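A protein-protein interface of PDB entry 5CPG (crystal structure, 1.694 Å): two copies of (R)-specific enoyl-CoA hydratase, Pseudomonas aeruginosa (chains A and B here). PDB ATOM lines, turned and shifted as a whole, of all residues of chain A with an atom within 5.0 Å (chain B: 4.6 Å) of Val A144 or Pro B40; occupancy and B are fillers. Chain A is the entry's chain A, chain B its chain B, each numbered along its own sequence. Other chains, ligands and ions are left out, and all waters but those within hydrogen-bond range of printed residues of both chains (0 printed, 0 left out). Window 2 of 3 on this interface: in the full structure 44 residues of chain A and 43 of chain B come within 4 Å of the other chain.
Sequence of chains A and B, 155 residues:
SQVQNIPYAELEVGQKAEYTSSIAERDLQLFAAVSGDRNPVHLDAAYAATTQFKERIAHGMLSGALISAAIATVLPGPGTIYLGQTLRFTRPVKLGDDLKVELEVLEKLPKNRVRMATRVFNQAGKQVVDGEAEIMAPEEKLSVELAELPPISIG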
ATOM      1  N   SER A   1     -28.141   7.450 -12.848  1.00  0.00           N
ATOM      2  CA  SER A   1     -26.696   7.269 -12.858  1.00  0.00           C
ATOM      3  C   SER A   1     -26.326   5.810 -13.083  1.00  0.00           C
ATOM      4  O   SER A   1     -27.182   4.916 -13.064  1.00  0.00           O
ATOM      5  CB  SER A   1     -26.076   7.755 -11.543  1.00  0.00           C
ATOM      6  OG  SER A   1     -26.593   9.023 -11.169  1.00  0.00           O
ATOM      7  N   GLN A   2     -25.041   5.574 -13.293  1.00  0.00           N
ATOM      8  CA  GLN A   2     -24.518   4.220 -13.350  1.00  0.00           C
ATOM      9  C   GLN A   2     -23.673   3.929 -12.122  1.00  0.00           C
ATOM     10  O   GLN A   2     -23.075   4.838 -11.535  1.00  0.00           O
ATOM     11  CB  GLN A   2     -23.702   4.021 -14.607  1.00  0.00           C
ATOM     12  CG  GLN A   2     -24.519   3.649 -15.787  1.00  0.00           C
ATOM     13  CD  GLN A   2     -23.645   3.076 -16.846  1.00  0.00           C
ATOM     14  OE1 GLN A   2     -22.428   3.267 -16.802  1.00  0.00           O
ATOM     15  NE2 GLN A   2     -24.235   2.346 -17.797  1.00  0.00           N
ATOM     16  N   VAL A   3     -23.633   2.656 -11.739  1.00  0.00           N
ATOM     17  CA  VAL A   3     -22.829   2.216 -10.608  1.00  0.00           C
ATOM     18  C   VAL A   3     -21.536   1.583 -11.106  1.00  0.00           C
ATOM     19  O   VAL A   3     -21.581   0.686 -11.943  1.00  0.00           O
ATOM     20  CB  VAL A   3     -23.621   1.211  -9.737  1.00  0.00           C
ATOM     21  CG1 VAL A   3     -22.752   0.691  -8.597  1.00  0.00           C
ATOM     22  CG2 VAL A   3     -24.856   1.900  -9.193  1.00  0.00           C
ATOM     23  N   PRO A  78     -20.941  -4.213  -8.698  1.00  0.00           N
ATOM     24  CA  PRO A  78     -21.284  -5.128  -9.801  1.00  0.00           C
ATOM     25  C   PRO A  78     -20.174  -6.088 -10.251  1.00  0.00           C
ATOM     26  O   PRO A  78     -19.031  -5.678 -10.381  1.00  0.00           O
ATOM     27  CB  PRO A  78     -21.660  -4.165 -10.928  1.00  0.00           C
ATOM     28  CG  PRO A  78     -22.238  -3.008 -10.216  1.00  0.00           C
ATOM     29  CD  PRO A  78     -21.436  -2.844  -8.941  1.00  0.00           C
ATOM     30  N   LEU A 142     -16.131  -2.166 -14.186  1.00  0.00           N
ATOM     31  CA  LEU A 142     -17.488  -2.321 -14.678  1.00  0.00           C
ATOM     32  C   LEU A 142     -18.340  -1.133 -14.316  1.00  0.00           C
ATOM     33  O   LEU A 142     -18.195  -0.556 -13.236  1.00  0.00           O
ATOM     34  CB  LEU A 142     -18.114  -3.578 -14.109  1.00  0.00           C
ATOM     35  CG  LEU A 142     -18.079  -4.832 -14.947  1.00  0.00           C
ATOM     36  CD1 LEU A 142     -18.403  -6.006 -14.047  1.00  0.00           C
ATOM     37  CD2 LEU A 142     -19.108  -4.679 -16.037  1.00  0.00           C
ATOM     38  N   SER A 143     -19.219  -0.763 -15.240  1.00  0.00           N
ATOM     39  CA  SER A 143     -20.199   0.291 -15.004  1.00  0.00           C
ATOM     40  C   SER A 143     -21.562  -0.270 -15.440  1.00  0.00           C
ATOM     41  O   SER A 143     -21.728  -0.757 -16.559  1.00  0.00           O
ATOM     42  CB  SER A 143     -19.828   1.565 -15.763  1.00  0.00           C
ATOM     43  OG  SER A 143     -20.380   2.719 -15.155  1.00  0.00           O
ATOM     44  N   VAL A 144     -22.527  -0.253 -14.533  1.00  0.00           N
ATOM     45  CA  VAL A 144     -23.764  -0.964 -14.781  1.00  0.00           C
ATOM     46  C   VAL A 144     -24.945  -0.080 -14.379  1.00  0.00           C
ATOM     47  O   VAL A 144     -24.899   0.586 -13.356  1.00  0.00           O
ATOM     48  CB  VAL A 144     -23.802  -2.294 -13.988  1.00  0.00           C
ATOM     49  CG1 VAL A 144     -25.149  -2.994 -14.144  1.00  0.00           C
ATOM     50  CG2 VAL A 144     -22.653  -3.205 -14.426  1.00  0.00           C
ATOM     51  N   GLU A 145     -25.978  -0.040 -15.214  1.00  0.00           N
ATOM     52  CA  GLU A 145     -27.199   0.654 -14.843  1.00  0.00           C
ATOM     53  C   GLU A 145     -28.016  -0.329 -14.009  1.00  0.00           C
ATOM     54  O   GLU A 145     -28.348  -1.413 -14.497  1.00  0.00           O
ATOM     55  CB  GLU A 145     -27.985   1.104 -16.088  1.00  0.00           C
ATOM     56  CG  GLU A 145     -29.245   1.910 -15.792  1.00  0.00           C
ATOM     57  CD  GLU A 145     -28.922   3.329 -15.349  1.00  0.00           C
ATOM     58  OE1 GLU A 145     -27.831   3.817 -15.709  1.00  0.00           O
ATOM     59  OE2 GLU A 145     -29.744   3.954 -14.640  1.00  0.00           O
ATOM     60  N   LEU A 146     -28.304   0.020 -12.763  1.00  0.00           N
ATOM     61  CA  LEU A 146     -29.203  -0.810 -11.965  1.00  0.00           C
ATOM     62  C   LEU A 146     -30.623  -0.770 -12.531  1.00  0.00           C
ATOM     63  O   LEU A 146     -31.052   0.243 -13.075  1.00  0.00           O
ATOM     64  CB  LEU A 146     -29.195  -0.366 -10.494  1.00  0.00           C
ATOM     65  CG  LEU A 146     -27.900  -0.469  -9.654  1.00  0.00           C
ATOM     66  CD1 LEU A 146     -28.149  -0.121  -8.183  1.00  0.00           C
ATOM     67  CD2 LEU A 146     -27.185  -1.822  -9.764  1.00  0.00           C
ATOM     68  N   ALA A 147     -31.364  -1.869 -12.401  1.00  0.00           N
ATOM     69  CA  ALA A 147     -32.704  -1.936 -12.982  1.00  0.00           C
ATOM     70  C   ALA A 147     -33.719  -1.157 -12.139  1.00  0.00           C
ATOM     71  O   ALA A 147     -33.743  -1.280 -10.918  1.00  0.00           O
ATOM     72  CB  ALA A 147     -33.154  -3.386 -13.125  1.00  0.00           C
ATOM     73  N   ARG B  38     -30.594  -4.094  -6.959  1.00  0.00           N
ATOM     74  CA  ARG B  38     -31.289  -4.096  -8.214  1.00  0.00           C
ATOM     75  C   ARG B  38     -30.347  -4.375  -9.378  1.00  0.00           C
ATOM     76  O   ARG B  38     -30.574  -3.879 -10.485  1.00  0.00           O
ATOM     77  CB  ARG B  38     -31.989  -2.750  -8.388  1.00  0.00           C
ATOM     78  CG  ARG B  38     -33.090  -2.566  -7.363  1.00  0.00           C
ATOM     79  CD  ARG B  38     -33.795  -1.207  -7.543  1.00  0.00           C
ATOM     80  NE  ARG B  38     -32.922  -0.125  -7.158  1.00  0.00           N
ATOM     81  CZ  ARG B  38     -32.393   0.752  -8.007  1.00  0.00           C
ATOM     82  NH1 ARG B  38     -32.688   0.702  -9.311  1.00  0.00           N
ATOM     83  NH2 ARG B  38     -31.594   1.698  -7.547  1.00  0.00           N
ATOM     84  N   ASN B  39     -29.329  -5.183  -9.144  1.00  0.00           N
ATOM     85  CA  ASN B  39     -28.464  -5.625 -10.267  1.00  0.00           C
ATOM     86  C   ASN B  39     -29.317  -6.285 -11.334  1.00  0.00           C
ATOM     87  O   ASN B  39     -30.233  -7.035 -11.015  1.00  0.00           O
ATOM     88  CB  ASN B  39     -27.381  -6.580  -9.759  1.00  0.00           C
ATOM     89  CG  ASN B  39     -26.166  -5.834  -9.210  1.00  0.00           C
ATOM     90  OD1 ASN B  39     -25.306  -5.394  -9.979  1.00  0.00           O
ATOM     91  ND2 ASN B  39     -26.111  -5.655  -7.896  1.00  0.00           N
ATOM     92  N   PRO B  40     -29.064  -5.984 -12.613  1.00  0.00           N
ATOM     93  CA  PRO B  40     -30.029  -6.407 -13.632  1.00  0.00           C
ATOM     94  C   PRO B  40     -30.077  -7.892 -13.922  1.00  0.00           C
ATOM     95  O   PRO B  40     -31.047  -8.320 -14.541  1.00  0.00           O
ATOM     96  CB  PRO B  40     -29.563  -5.634 -14.900  1.00  0.00           C
ATOM     97  CG  PRO B  40     -28.144  -5.361 -14.664  1.00  0.00           C
ATOM     98  CD  PRO B  40     -28.054  -5.057 -13.167  1.00  0.00           C
ATOM     99  N   VAL B  41     -29.089  -8.674 -13.486  1.00  0.00           N
ATOM    100  CA  VAL B  41     -29.163 -10.098 -13.708  1.00  0.00           C
ATOM    101  C   VAL B  41     -30.346 -10.647 -12.883  1.00  0.00           C
ATOM    102  O   VAL B  41     -30.807 -11.744 -13.126  1.00  0.00           O
ATOM    103  CB  VAL B  41     -27.838 -10.817 -13.306  1.00  0.00           C
ATOM    104  CG1 VAL B  41     -27.742 -11.011 -11.760  1.00  0.00           C
ATOM    105  CG2 VAL B  41     -27.736 -12.174 -13.991  1.00  0.00           C
ATOM    106  N   HIS B  42     -30.811  -9.893 -11.882  1.00  0.00           N
ATOM    107  CA  HIS B  42     -31.891 -10.418 -11.051  1.00  0.00           C
ATOM    108  C   HIS B  42     -33.244  -9.993 -11.580  1.00  0.00           C
ATOM    109  O   HIS B  42     -34.265 -10.584 -11.211  1.00  0.00           O
ATOM    110  CB  HIS B  42     -31.757  -9.957  -9.580  1.00  0.00           C
ATOM    111  CG  HIS B  42     -30.467 -10.363  -8.939  1.00  0.00           C
ATOM    112  ND1 HIS B  42     -30.080 -11.683  -8.818  1.00  0.00           N
ATOM    113  CD2 HIS B  42     -29.472  -9.619  -8.397  1.00  0.00           C
ATOM    114  CE1 HIS B  42     -28.887 -11.730  -8.235  1.00  0.00           C
ATOM    115  NE2 HIS B  42     -28.506 -10.492  -7.957  1.00  0.00           N
ATOM    116  N   LEU B  43     -33.279  -8.977 -12.436  1.00  0.00           N
ATOM    117  CA  LEU B  43     -34.539  -8.271 -12.728  1.00  0.00           C
ATOM    118  C   LEU B  43     -34.895  -8.102 -14.210  1.00  0.00           C
ATOM    119  O   LEU B  43     -36.073  -8.065 -14.551  1.00  0.00           O
ATOM    120  CB  LEU B  43     -34.516  -6.874 -12.109  1.00  0.00           C
ATOM    121  CG  LEU B  43     -34.437  -6.883 -10.567  1.00  0.00           C
ATOM    122  CD1 LEU B  43     -34.247  -5.480 -10.038  1.00  0.00           C
ATOM    123  CD2 LEU B  43     -35.715  -7.471 -10.010  1.00  0.00           C
ATOM    124  N   ASP B  44     -33.878  -7.954 -15.057  1.00  0.00           N
ATOM    125  CA  ASP B  44     -34.034  -7.543 -16.457  1.00  0.00           C
ATOM    126  C   ASP B  44     -33.862  -8.771 -17.332  1.00  0.00           C
ATOM    127  O   ASP B  44     -32.745  -9.276 -17.457  1.00  0.00           O
ATOM    128  CB  ASP B  44     -32.989  -6.433 -16.792  1.00  0.00           C
ATOM    129  CG  ASP B  44     -33.090  -5.914 -18.229  1.00  0.00           C
ATOM    130  OD1 ASP B  44     -33.467  -6.675 -19.150  1.00  0.00           O
ATOM    131  OD2 ASP B  44     -32.719  -4.746 -18.435  1.00  0.00           O
ATOM    132  N   TYR B  47     -31.494  -8.440 -20.336  1.00  0.00           N
ATOM    133  CA  TYR B  47     -30.105  -8.440 -19.920  1.00  0.00           C
ATOM    134  C   TYR B  47     -29.604  -9.830 -19.556  1.00  0.00           C
ATOM    135  O   TYR B  47     -28.528 -10.259 -19.971  1.00  0.00           O
ATOM    136  CB  TYR B  47     -29.890  -7.483 -18.725  1.00  0.00           C
ATOM    137  CG  TYR B  47     -28.507  -7.640 -18.163  1.00  0.00           C
ATOM    138  CD1 TYR B  47     -28.264  -8.444 -17.057  1.00  0.00           C
ATOM    139  CD2 TYR B  47     -27.423  -6.985 -18.753  1.00  0.00           C
ATOM    140  CE1 TYR B  47     -26.989  -8.633 -16.564  1.00  0.00           C
ATOM    141  CE2 TYR B  47     -26.138  -7.152 -18.246  1.00  0.00           C
ATOM    142  CZ  TYR B  47     -25.935  -7.978 -17.160  1.00  0.00           C
ATOM    143  OH  TYR B  47     -24.670  -8.161 -16.663  1.00  0.00           O
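OD1 of Asn B39 touches CG of Pro A78, at 3.9 Å.
CG1 of Val A144 touches CD of Pro B40, at 3.7 Å.
Glu A145 touches Pro B40.
Arg B38 touches Leu A146.
CB of Leu B43 touches CB of Ala A147 (3.9 Å).
Of the 8 printed residues of chain B, 4 touch a printed residue of chain A.
Printed residues of chain B that touch a printed residue of chain A: Arg B38, Asn B39, Pro B40 and Leu B43.
Of the 10 printed residues of chain A, 5 touch a printed residue of chain B.
Hydrophobic or aromatic side chains of chain A within 4 Å of the printed part of chain B: Pro A78, Val A144, Leu A146 and Ala A147.
Among the printed residues, no Asp or Glu carboxylate lies within 4 Å of a Lys or Arg side-chain nitrogen of the other chain.
Val A3 touches none of the printed residues of chain B.
Of chain B, only Pro B40 (3.7 Å) comes within 4 Å of Val A144.
Printed residues of chain B within 4 Å of Leu A146: Arg B38.
Of the printed residues of chain B, Ala A147 touches Arg B38 and Leu B43.
Val B41 touches none of the printed residues of chain A.
The nearest printed residue of chain B that does not touch Val A144 is Asn B39 (4.8 Å).
The nearest printed residue of chain A that does not touch Asn B39 is Leu A146 (4.03 Å).
No position is printed for both chains.
The backbone carbonyl oxygen (O) of Val A3 sits at hydrogen-bond distance from the backbone NH (N) of Val A144, 2.9 Å away.
NH1 of Arg B38 lies within hydrogen-bond range of O of Ala A147 (2.8 Å).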
